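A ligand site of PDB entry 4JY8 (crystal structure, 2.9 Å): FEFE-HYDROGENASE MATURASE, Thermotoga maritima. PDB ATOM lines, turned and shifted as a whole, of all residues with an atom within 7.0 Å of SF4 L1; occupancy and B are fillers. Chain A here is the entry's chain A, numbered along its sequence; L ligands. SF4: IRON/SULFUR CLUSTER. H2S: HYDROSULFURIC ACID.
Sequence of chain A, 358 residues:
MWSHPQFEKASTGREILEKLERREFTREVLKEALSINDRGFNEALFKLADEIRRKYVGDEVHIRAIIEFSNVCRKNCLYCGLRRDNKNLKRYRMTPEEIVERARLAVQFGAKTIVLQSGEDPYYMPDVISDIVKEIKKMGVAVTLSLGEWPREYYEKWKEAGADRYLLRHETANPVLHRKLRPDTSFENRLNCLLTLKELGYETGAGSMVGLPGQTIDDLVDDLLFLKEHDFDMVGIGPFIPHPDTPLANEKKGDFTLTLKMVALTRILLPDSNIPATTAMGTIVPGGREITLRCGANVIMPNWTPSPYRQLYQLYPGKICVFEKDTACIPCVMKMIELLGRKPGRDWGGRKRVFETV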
ATOM      1  N   ASN A  71      22.710  11.926  -5.651  1.00  0.00           N
ATOM      2  CA  ASN A  71      22.802  12.341  -7.035  1.00  0.00           C
ATOM      3  C   ASN A  71      24.030  13.152  -7.380  1.00  0.00           C
ATOM      4  O   ASN A  71      24.044  13.854  -8.391  1.00  0.00           O
ATOM      5  CB  ASN A  71      21.556  13.132  -7.418  1.00  0.00           C
ATOM      6  CG  ASN A  71      21.484  14.480  -6.730  1.00  0.00           C
ATOM      7  OD1 ASN A  71      22.281  14.771  -5.837  1.00  0.00           O
ATOM      8  ND2 ASN A  71      20.578  15.335  -7.162  1.00  0.00           N
ATOM      9  N   VAL A  72      25.054  13.039  -6.552  1.00  0.00           N
ATOM     10  CA  VAL A  72      26.358  13.595  -6.856  1.00  0.00           C
ATOM     11  C   VAL A  72      27.094  12.672  -7.801  1.00  0.00           C
ATOM     12  O   VAL A  72      27.181  11.486  -7.535  1.00  0.00           O
ATOM     13  CB  VAL A  72      27.151  13.815  -5.560  1.00  0.00           C
ATOM     14  CG1 VAL A  72      28.579  14.158  -5.866  1.00  0.00           C
ATOM     15  CG2 VAL A  72      26.441  14.838  -4.658  1.00  0.00           C
ATOM     16  N   CYS A  73      27.685  13.217  -8.859  1.00  0.00           N
ATOM     17  CA  CYS A  73      28.519  12.423  -9.747  1.00  0.00           C
ATOM     18  C   CYS A  73      29.743  13.200 -10.124  1.00  0.00           C
ATOM     19  O   CYS A  73      29.695  14.409 -10.395  1.00  0.00           O
ATOM     20  CB  CYS A  73      27.728  11.983 -10.960  1.00  0.00           C
ATOM     21  SG  CYS A  73      28.484  10.686 -11.933  1.00  0.00           S
ATOM     22  N   ARG A  74      30.871  12.483 -10.155  1.00  0.00           N
ATOM     23  CA  ARG A  74      32.194  12.967 -10.593  1.00  0.00           C
ATOM     24  C   ARG A  74      32.494  12.920 -12.075  1.00  0.00           C
ATOM     25  O   ARG A  74      33.451  13.527 -12.567  1.00  0.00           O
ATOM     26  CB  ARG A  74      33.257  12.178  -9.821  1.00  0.00           C
ATOM     27  CG  ARG A  74      33.376  10.657 -10.195  1.00  0.00           C
ATOM     28  CD  ARG A  74      34.396   9.931  -9.278  1.00  0.00           C
ATOM     29  NE  ARG A  74      34.530   8.475  -9.470  1.00  0.00           N
ATOM     30  CZ  ARG A  74      35.390   7.864 -10.288  1.00  0.00           C
ATOM     31  NH1 ARG A  74      36.225   8.562 -11.053  1.00  0.00           N
ATOM     32  NH2 ARG A  74      35.364   6.529 -10.367  1.00  0.00           N
ATOM     33  N   LYS A  75      31.677  12.168 -12.783  1.00  0.00           N
ATOM     34  CA  LYS A  75      31.860  11.959 -14.200  1.00  0.00           C
ATOM     35  C   LYS A  75      30.981  12.965 -14.925  1.00  0.00           C
ATOM     36  O   LYS A  75      30.233  13.726 -14.295  1.00  0.00           O
ATOM     37  CB  LYS A  75      31.589  10.494 -14.625  1.00  0.00           C
ATOM     38  CG  LYS A  75      32.779   9.536 -14.361  1.00  0.00           C
ATOM     39  CD  LYS A  75      32.515   8.146 -14.923  1.00  0.00           C
ATOM     40  CE  LYS A  75      33.741   7.182 -15.035  1.00  0.00           C
ATOM     41  NZ  LYS A  75      34.562   6.907 -13.787  1.00  0.00           N
ATOM     42  N   ASN A  76      31.125  13.026 -16.241  1.00  0.00           N
ATOM     43  CA  ASN A  76      30.488  14.027 -17.052  1.00  0.00           C
ATOM     44  C   ASN A  76      29.775  13.480 -18.300  1.00  0.00           C
ATOM     45  O   ASN A  76      29.768  14.137 -19.338  1.00  0.00           O
ATOM     46  CB  ASN A  76      31.547  15.028 -17.486  1.00  0.00           C
ATOM     47  CG  ASN A  76      30.994  16.411 -17.687  1.00  0.00           C
ATOM     48  OD1 ASN A  76      29.956  16.761 -17.105  1.00  0.00           O
ATOM     49  ND2 ASN A  76      31.604  17.180 -18.608  1.00  0.00           N
ATOM     50  N   CYS A  77      29.155  12.304 -18.176  1.00  0.00           N
ATOM     51  CA  CYS A  77      28.485  11.678 -19.294  1.00  0.00           C
ATOM     52  C   CYS A  77      27.501  12.619 -19.978  1.00  0.00           C
ATOM     53  O   CYS A  77      26.867  13.441 -19.322  1.00  0.00           O
ATOM     54  CB  CYS A  77      27.774  10.400 -18.834  1.00  0.00           C
ATOM     55  SG  CYS A  77      28.818   9.251 -18.025  1.00  0.00           S
ATOM     56  N   LEU A  78      27.520  12.638 -21.293  1.00  0.00           N
ATOM     57  CA  LEU A  78      26.787  13.651 -22.019  1.00  0.00           C
ATOM     58  C   LEU A  78      25.247  13.507 -22.004  1.00  0.00           C
ATOM     59  O   LEU A  78      24.543  14.515 -22.179  1.00  0.00           O
ATOM     60  CB  LEU A  78      27.235  13.667 -23.471  1.00  0.00           C
ATOM     61  CG  LEU A  78      28.466  14.510 -23.819  1.00  0.00           C
ATOM     62  CD1 LEU A  78      29.664  14.038 -22.997  1.00  0.00           C
ATOM     63  CD2 LEU A  78      28.774  14.481 -25.287  1.00  0.00           C
ATOM     64  N   TYR A  79      24.726  12.273 -21.802  1.00  0.00           N
ATOM     65  CA  TYR A  79      23.280  12.002 -21.874  1.00  0.00           C
ATOM     66  C   TYR A  79      22.638  12.250 -20.545  1.00  0.00           C
ATOM     67  O   TYR A  79      21.416  12.280 -20.444  1.00  0.00           O
ATOM     68  CB  TYR A  79      22.995  10.557 -22.296  1.00  0.00           C
ATOM     69  CG  TYR A  79      23.808   9.519 -21.627  1.00  0.00           C
ATOM     70  CD1 TYR A  79      23.460   9.078 -20.364  1.00  0.00           C
ATOM     71  CD2 TYR A  79      24.963   9.018 -22.196  1.00  0.00           C
ATOM     72  CE1 TYR A  79      24.193   8.133 -19.725  1.00  0.00           C
ATOM     73  CE2 TYR A  79      25.733   8.086 -21.538  1.00  0.00           C
ATOM     74  CZ  TYR A  79      25.343   7.635 -20.303  1.00  0.00           C
ATOM     75  OH  TYR A  79      26.104   6.698 -19.617  1.00  0.00           O
ATOM     76  N   CYS A  80      23.460  12.355 -19.498  1.00  0.00           N
ATOM     77  CA  CYS A  80      22.955  12.148 -18.148  1.00  0.00           C
ATOM     78  C   CYS A  80      22.707  13.453 -17.380  1.00  0.00           C
ATOM     79  O   CYS A  80      23.558  14.323 -17.248  1.00  0.00           O
ATOM     80  CB  CYS A  80      23.997  11.327 -17.325  1.00  0.00           C
ATOM     81  SG  CYS A  80      23.535  10.801 -15.574  1.00  0.00           S
ATOM     82  N   GLY A  81      21.500  13.530 -16.836  1.00  0.00           N
ATOM     83  CA  GLY A  81      21.121  14.645 -16.017  1.00  0.00           C
ATOM     84  C   GLY A  81      21.969  14.797 -14.777  1.00  0.00           C
ATOM     85  O   GLY A  81      22.031  15.889 -14.206  1.00  0.00           O
ATOM     86  N   LEU A  82      22.665  13.729 -14.375  1.00  0.00           N
ATOM     87  CA  LEU A  82      23.529  13.823 -13.212  1.00  0.00           C
ATOM     88  C   LEU A  82      24.956  14.260 -13.485  1.00  0.00           C
ATOM     89  O   LEU A  82      25.732  14.460 -12.549  1.00  0.00           O
ATOM     90  CB  LEU A  82      23.599  12.471 -12.469  1.00  0.00           C
ATOM     91  CG  LEU A  82      22.413  11.699 -11.907  1.00  0.00           C
ATOM     92  CD1 LEU A  82      23.018  10.636 -11.072  1.00  0.00           C
ATOM     93  CD2 LEU A  82      21.508  12.535 -11.035  1.00  0.00           C
ATOM     94  N   ARG A  83      25.267  14.514 -14.740  1.00  0.00           N
ATOM     95  CA  ARG A  83      26.646  14.850 -15.102  1.00  0.00           C
ATOM     96  C   ARG A  83      27.174  16.009 -14.267  1.00  0.00           C
ATOM     97  O   ARG A  83      26.427  16.903 -13.860  1.00  0.00           O
ATOM     98  CB  ARG A  83      26.678  15.194 -16.596  1.00  0.00           C
ATOM     99  CG  ARG A  83      25.858  16.430 -16.964  1.00  0.00           C
ATOM    100  CD  ARG A  83      25.632  16.438 -18.452  1.00  0.00           C
ATOM    101  NE  ARG A  83      26.897  16.266 -19.135  1.00  0.00           N
ATOM    102  CZ  ARG A  83      27.673  17.285 -19.527  1.00  0.00           C
ATOM    103  NH1 ARG A  83      27.289  18.553 -19.308  1.00  0.00           N
ATOM    104  NH2 ARG A  83      28.815  17.046 -20.171  1.00  0.00           N
ATOM    105  N   ARG A  84      28.472  15.999 -14.006  1.00  0.00           N
ATOM    106  CA  ARG A  84      29.029  17.003 -13.106  1.00  0.00           C
ATOM    107  C   ARG A  84      28.798  18.457 -13.561  1.00  0.00           C
ATOM    108  O   ARG A  84      28.532  19.296 -12.708  1.00  0.00           O
ATOM    109  CB  ARG A  84      30.519  16.718 -12.786  1.00  0.00           C
ATOM    110  CG  ARG A  84      31.483  16.958 -13.926  1.00  0.00           C
ATOM    111  CD  ARG A  84      32.961  16.800 -13.471  1.00  0.00           C
ATOM    112  NE  ARG A  84      33.872  16.979 -14.613  1.00  0.00           N
ATOM    113  CZ  ARG A  84      34.353  16.001 -15.374  1.00  0.00           C
ATOM    114  NH1 ARG A  84      34.170  14.733 -15.046  1.00  0.00           N
ATOM    115  NH2 ARG A  84      35.053  16.307 -16.469  1.00  0.00           N
ATOM    116  N   SER A 118      23.460   5.265  -7.396  1.00  0.00           N
ATOM    117  CA  SER A 118      23.874   6.661  -7.359  1.00  0.00           C
ATOM    118  C   SER A 118      24.640   7.028  -8.594  1.00  0.00           C
ATOM    119  O   SER A 118      25.007   6.152  -9.399  1.00  0.00           O
ATOM    120  CB  SER A 118      24.726   6.949  -6.148  1.00  0.00           C
ATOM    121  OG  SER A 118      25.895   6.160  -6.216  1.00  0.00           O
ATOM    122  N   GLY A 119      24.853   8.341  -8.744  1.00  0.00           N
ATOM    123  CA  GLY A 119      25.950   8.882  -9.524  1.00  0.00           C
ATOM    124  C   GLY A 119      27.234   8.365  -8.914  1.00  0.00           C
ATOM    125  O   GLY A 119      27.228   7.870  -7.802  1.00  0.00           O
ATOM    126  N   GLU A 120      28.364   8.516  -9.603  1.00  0.00           N
ATOM    127  CA  GLU A 120      29.630   8.127  -8.988  1.00  0.00           C
ATOM    128  C   GLU A 120      30.133   9.108  -7.906  1.00  0.00           C
ATOM    129  O   GLU A 120      30.930   9.989  -8.186  1.00  0.00           O
ATOM    130  CB  GLU A 120      30.704   7.954 -10.066  1.00  0.00           C
ATOM    131  CG  GLU A 120      30.474   6.790 -11.022  1.00  0.00           C
ATOM    132  CD  GLU A 120      31.696   6.430 -11.863  1.00  0.00           C
ATOM    133  OE1 GLU A 120      32.784   7.034 -11.623  1.00  0.00           O
ATOM    134  OE2 GLU A 120      31.561   5.549 -12.757  1.00  0.00           O
ATOM    135  N   LEU A 147      26.584   1.684  -8.637  1.00  0.00           N
ATOM    136  CA  LEU A 147      27.391   2.797  -8.179  1.00  0.00           C
ATOM    137  C   LEU A 147      28.377   3.305  -9.231  1.00  0.00           C
ATOM    138  O   LEU A 147      29.186   4.203  -8.943  1.00  0.00           O
ATOM    139  CB  LEU A 147      28.090   2.433  -6.876  1.00  0.00           C
ATOM    140  CG  LEU A 147      27.171   1.851  -5.791  1.00  0.00           C
ATOM    141  CD1 LEU A 147      27.998   1.515  -4.543  1.00  0.00           C
ATOM    142  CD2 LEU A 147      25.982   2.740  -5.435  1.00  0.00           C
ATOM    143  N   GLY A 148      28.416   2.698 -10.417  1.00  0.00           N
ATOM    144  CA  GLY A 148      29.383   3.102 -11.431  1.00  0.00           C
ATOM    145  C   GLY A 148      30.689   2.337 -11.452  1.00  0.00           C
ATOM    146  O   GLY A 148      30.759   1.188 -11.005  1.00  0.00           O
ATOM    147  N   GLU A 149      31.720   2.957 -12.021  1.00  0.00           N
ATOM    148  CA  GLU A 149      33.002   2.319 -12.239  1.00  0.00           C
ATOM    149  C   GLU A 149      33.946   2.599 -11.050  1.00  0.00           C
ATOM    150  O   GLU A 149      34.197   3.749 -10.658  1.00  0.00           O
ATOM    151  CB  GLU A 149      33.582   2.889 -13.525  1.00  0.00           C
ATOM    152  CG  GLU A 149      32.771   2.518 -14.728  1.00  0.00           C
ATOM    153  CD  GLU A 149      33.203   3.247 -15.981  1.00  0.00           C
ATOM    154  OE1 GLU A 149      34.426   3.494 -16.134  1.00  0.00           O
ATOM    155  OE2 GLU A 149      32.324   3.565 -16.803  1.00  0.00           O
ATOM    156  N   GLU A 171      25.731   0.625 -21.826  1.00  0.00           N
ATOM    157  CA  GLU A 171      25.217   1.810 -22.552  1.00  0.00           C
ATOM    158  C   GLU A 171      25.412   1.696 -24.079  1.00  0.00           C
ATOM    159  O   GLU A 171      24.439   1.827 -24.822  1.00  0.00           O
ATOM    160  CB  GLU A 171      25.835   3.141 -22.053  1.00  0.00           C
ATOM    161  CG  GLU A 171      25.898   3.369 -20.523  1.00  0.00           C
ATOM    162  CD  GLU A 171      24.517   3.437 -19.817  1.00  0.00           C
ATOM    163  OE1 GLU A 171      23.452   3.241 -20.444  1.00  0.00           O
ATOM    164  OE2 GLU A 171      24.501   3.740 -18.601  1.00  0.00           O
ATOM    165  N   LEU A 181      30.589   9.858 -25.703  1.00  0.00           N
ATOM    166  CA  LEU A 181      29.512  10.089 -24.725  1.00  0.00           C
ATOM    167  C   LEU A 181      29.950  10.058 -23.239  1.00  0.00           C
ATOM    168  O   LEU A 181      29.256  10.583 -22.380  1.00  0.00           O
ATOM    169  CB  LEU A 181      28.423   9.044 -24.931  1.00  0.00           C
ATOM    170  CG  LEU A 181      27.716   9.237 -26.274  1.00  0.00           C
ATOM    171  CD1 LEU A 181      26.730   8.095 -26.562  1.00  0.00           C
ATOM    172  CD2 LEU A 181      27.018  10.605 -26.308  1.00  0.00           C
ATOM    173  N   ARG A 182      31.090   9.422 -22.947  1.00  0.00           N
ATOM    174  CA  ARG A 182      31.499   9.221 -21.561  1.00  0.00           C
ATOM    175  C   ARG A 182      32.992   9.511 -21.498  1.00  0.00           C
ATOM    176  O   ARG A 182      33.799   8.630 -21.258  1.00  0.00           O
ATOM    177  CB  ARG A 182      31.199   7.781 -21.086  1.00  0.00           C
ATOM    178  CG  ARG A 182      29.783   7.385 -21.291  1.00  0.00           C
ATOM    179  CD  ARG A 182      29.366   6.100 -20.621  1.00  0.00           C
ATOM    180  NE  ARG A 182      29.308   6.224 -19.162  1.00  0.00           N
ATOM    181  CZ  ARG A 182      30.120   5.645 -18.278  1.00  0.00           C
ATOM    182  NH1 ARG A 182      30.979   4.696 -18.662  1.00  0.00           N
ATOM    183  NH2 ARG A 182      30.038   5.989 -16.998  1.00  0.00           N
ATOM    184  N   ASP A 184      35.048  10.541 -19.584  1.00  0.00           N
ATOM    185  CA  ASP A 184      35.866  10.197 -18.431  1.00  0.00           C
ATOM    186  C   ASP A 184      36.479   8.842 -18.512  1.00  0.00           C
ATOM    187  O   ASP A 184      37.419   8.532 -17.797  1.00  0.00           O
ATOM    188  CB  ASP A 184      35.031  10.267 -17.154  1.00  0.00           C
ATOM    189  CG  ASP A 184      34.254  11.557 -17.033  1.00  0.00           C
ATOM    190  OD1 ASP A 184      34.851  12.617 -16.708  1.00  0.00           O
ATOM    191  OD2 ASP A 184      33.014  11.486 -17.247  1.00  0.00           O
ATOM    192  N   ARG A 190      34.883   0.053 -19.064  1.00  0.00           N
ATOM    193  CA  ARG A 190      33.574  -0.476 -18.699  1.00  0.00           C
ATOM    194  C   ARG A 190      33.565  -2.020 -18.773  1.00  0.00           C
ATOM    195  O   ARG A 190      33.134  -2.732 -17.831  1.00  0.00           O
ATOM    196  CB  ARG A 190      32.497   0.120 -19.624  1.00  0.00           C
ATOM    197  CG  ARG A 190      31.077   0.009 -19.113  1.00  0.00           C
ATOM    198  CD  ARG A 190      30.797   1.128 -18.121  1.00  0.00           C
ATOM    199  NE  ARG A 190      29.375   1.235 -17.814  1.00  0.00           N
ATOM    200  CZ  ARG A 190      28.857   2.050 -16.904  1.00  0.00           C
ATOM    201  NH1 ARG A 190      29.642   2.925 -16.257  1.00  0.00           N
ATOM    202  NH2 ARG A 190      27.551   2.017 -16.665  1.00  0.00           N
ATOM    203  N   MET A 209      21.366   1.775 -23.954  1.00  0.00           N
ATOM    204  CA  MET A 209      20.303   2.630 -24.389  1.00  0.00           C
ATOM    205  C   MET A 209      20.171   2.455 -25.885  1.00  0.00           C
ATOM    206  O   MET A 209      21.140   2.132 -26.574  1.00  0.00           O
ATOM    207  CB  MET A 209      20.548   4.086 -24.024  1.00  0.00           C
ATOM    208  CG  MET A 209      20.389   4.410 -22.559  1.00  0.00           C
ATOM    209  SD  MET A 209      20.917   6.104 -22.236  1.00  0.00           S
ATOM    210  CE  MET A 209      22.696   5.895 -22.305  1.00  0.00           C
HETATM  211 FE1  SF4 L   1      27.850   8.797 -16.091  1.00  0.00          FE
HETATM  212 FE2  SF4 L   1      26.318   7.397 -14.246  1.00  0.00          FE
HETATM  213 FE3  SF4 L   1      27.513   9.738 -13.621  1.00  0.00          FE
HETATM  214 FE4  SF4 L   1      25.351   9.661 -15.189  1.00  0.00          FE
HETATM  215  S1  SF4 L   1      25.401   9.110 -12.976  1.00  0.00           S
HETATM  216  S2  SF4 L   1      27.254  10.955 -15.521  1.00  0.00           S
HETATM  217  S3  SF4 L   1      25.818   7.809 -16.452  1.00  0.00           S
HETATM  218  S4  SF4 L   1      28.580   7.765 -14.206  1.00  0.00           S
HETATM  219  S   H2S L   2      25.851   4.497 -12.728  1.00  0.00           S
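Residues that only touch SF4 L1: Leu 82 (3.4 Å), Gly 119 (3.5 Å), Glu 120 (3.8 Å) and Arg 83 (3.96 Å).
Hydrophobic or aromatic side chains that line SF4 L1: Tyr 79 and Leu 82.
The nearest printed residue that does not touch SF4 L1 is Lys 75 (4.02 Å).
An iron atom (FE3) of SF4 L1 is bound by the side-chain sulfur (SG) of Cys 73, 2.2 Å away.
An iron atom (FE4) of SF4 L1 is bound by the side-chain sulfur of Cys 80.
The backbone NH (N) of Cys 77 sits close to a sulfur (S2) of SF4 L1, 3.5 Å away.
FE1 of SF4 L1 is bound by SG of Cys 77.
The side-chain hydroxyl of Tyr 79 sits close to a sulfur (S3) of SF4 L1 (3.4 Å).
The guanidinium group of Arg 182 lies close to a sulfur (S4) of SF4 L1 (3.6 Å).
The backbone NH of Glu 120 sits close to the side-chain sulfur of Cys 73.
N of Lys 75 lies close to SG of Cys 73.
SG of Cys 80 sits close to N of Leu 82.
NE of Arg 182 sits close to SG of Cys 77, at 3.3 Å.
The backbone carbonyl oxygen (O) of Cys 77 sits at hydrogen-bond distance from the guanidinium group (NE) of Arg 83, at 2.8 Å.
The side-chain carboxylate (OE1) of Glu 120 is in salt-bridge range of the side-chain amino group (NZ) of Lys 75 (2.8 Å).
The guanidinium group of Arg 74 lies within salt-bridge range of the side-chain carboxylate of Glu 120 (2.9 Å).
O of Asn 76 is in hydrogen-bond range of NH2 of Arg 83 (3.2 Å).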
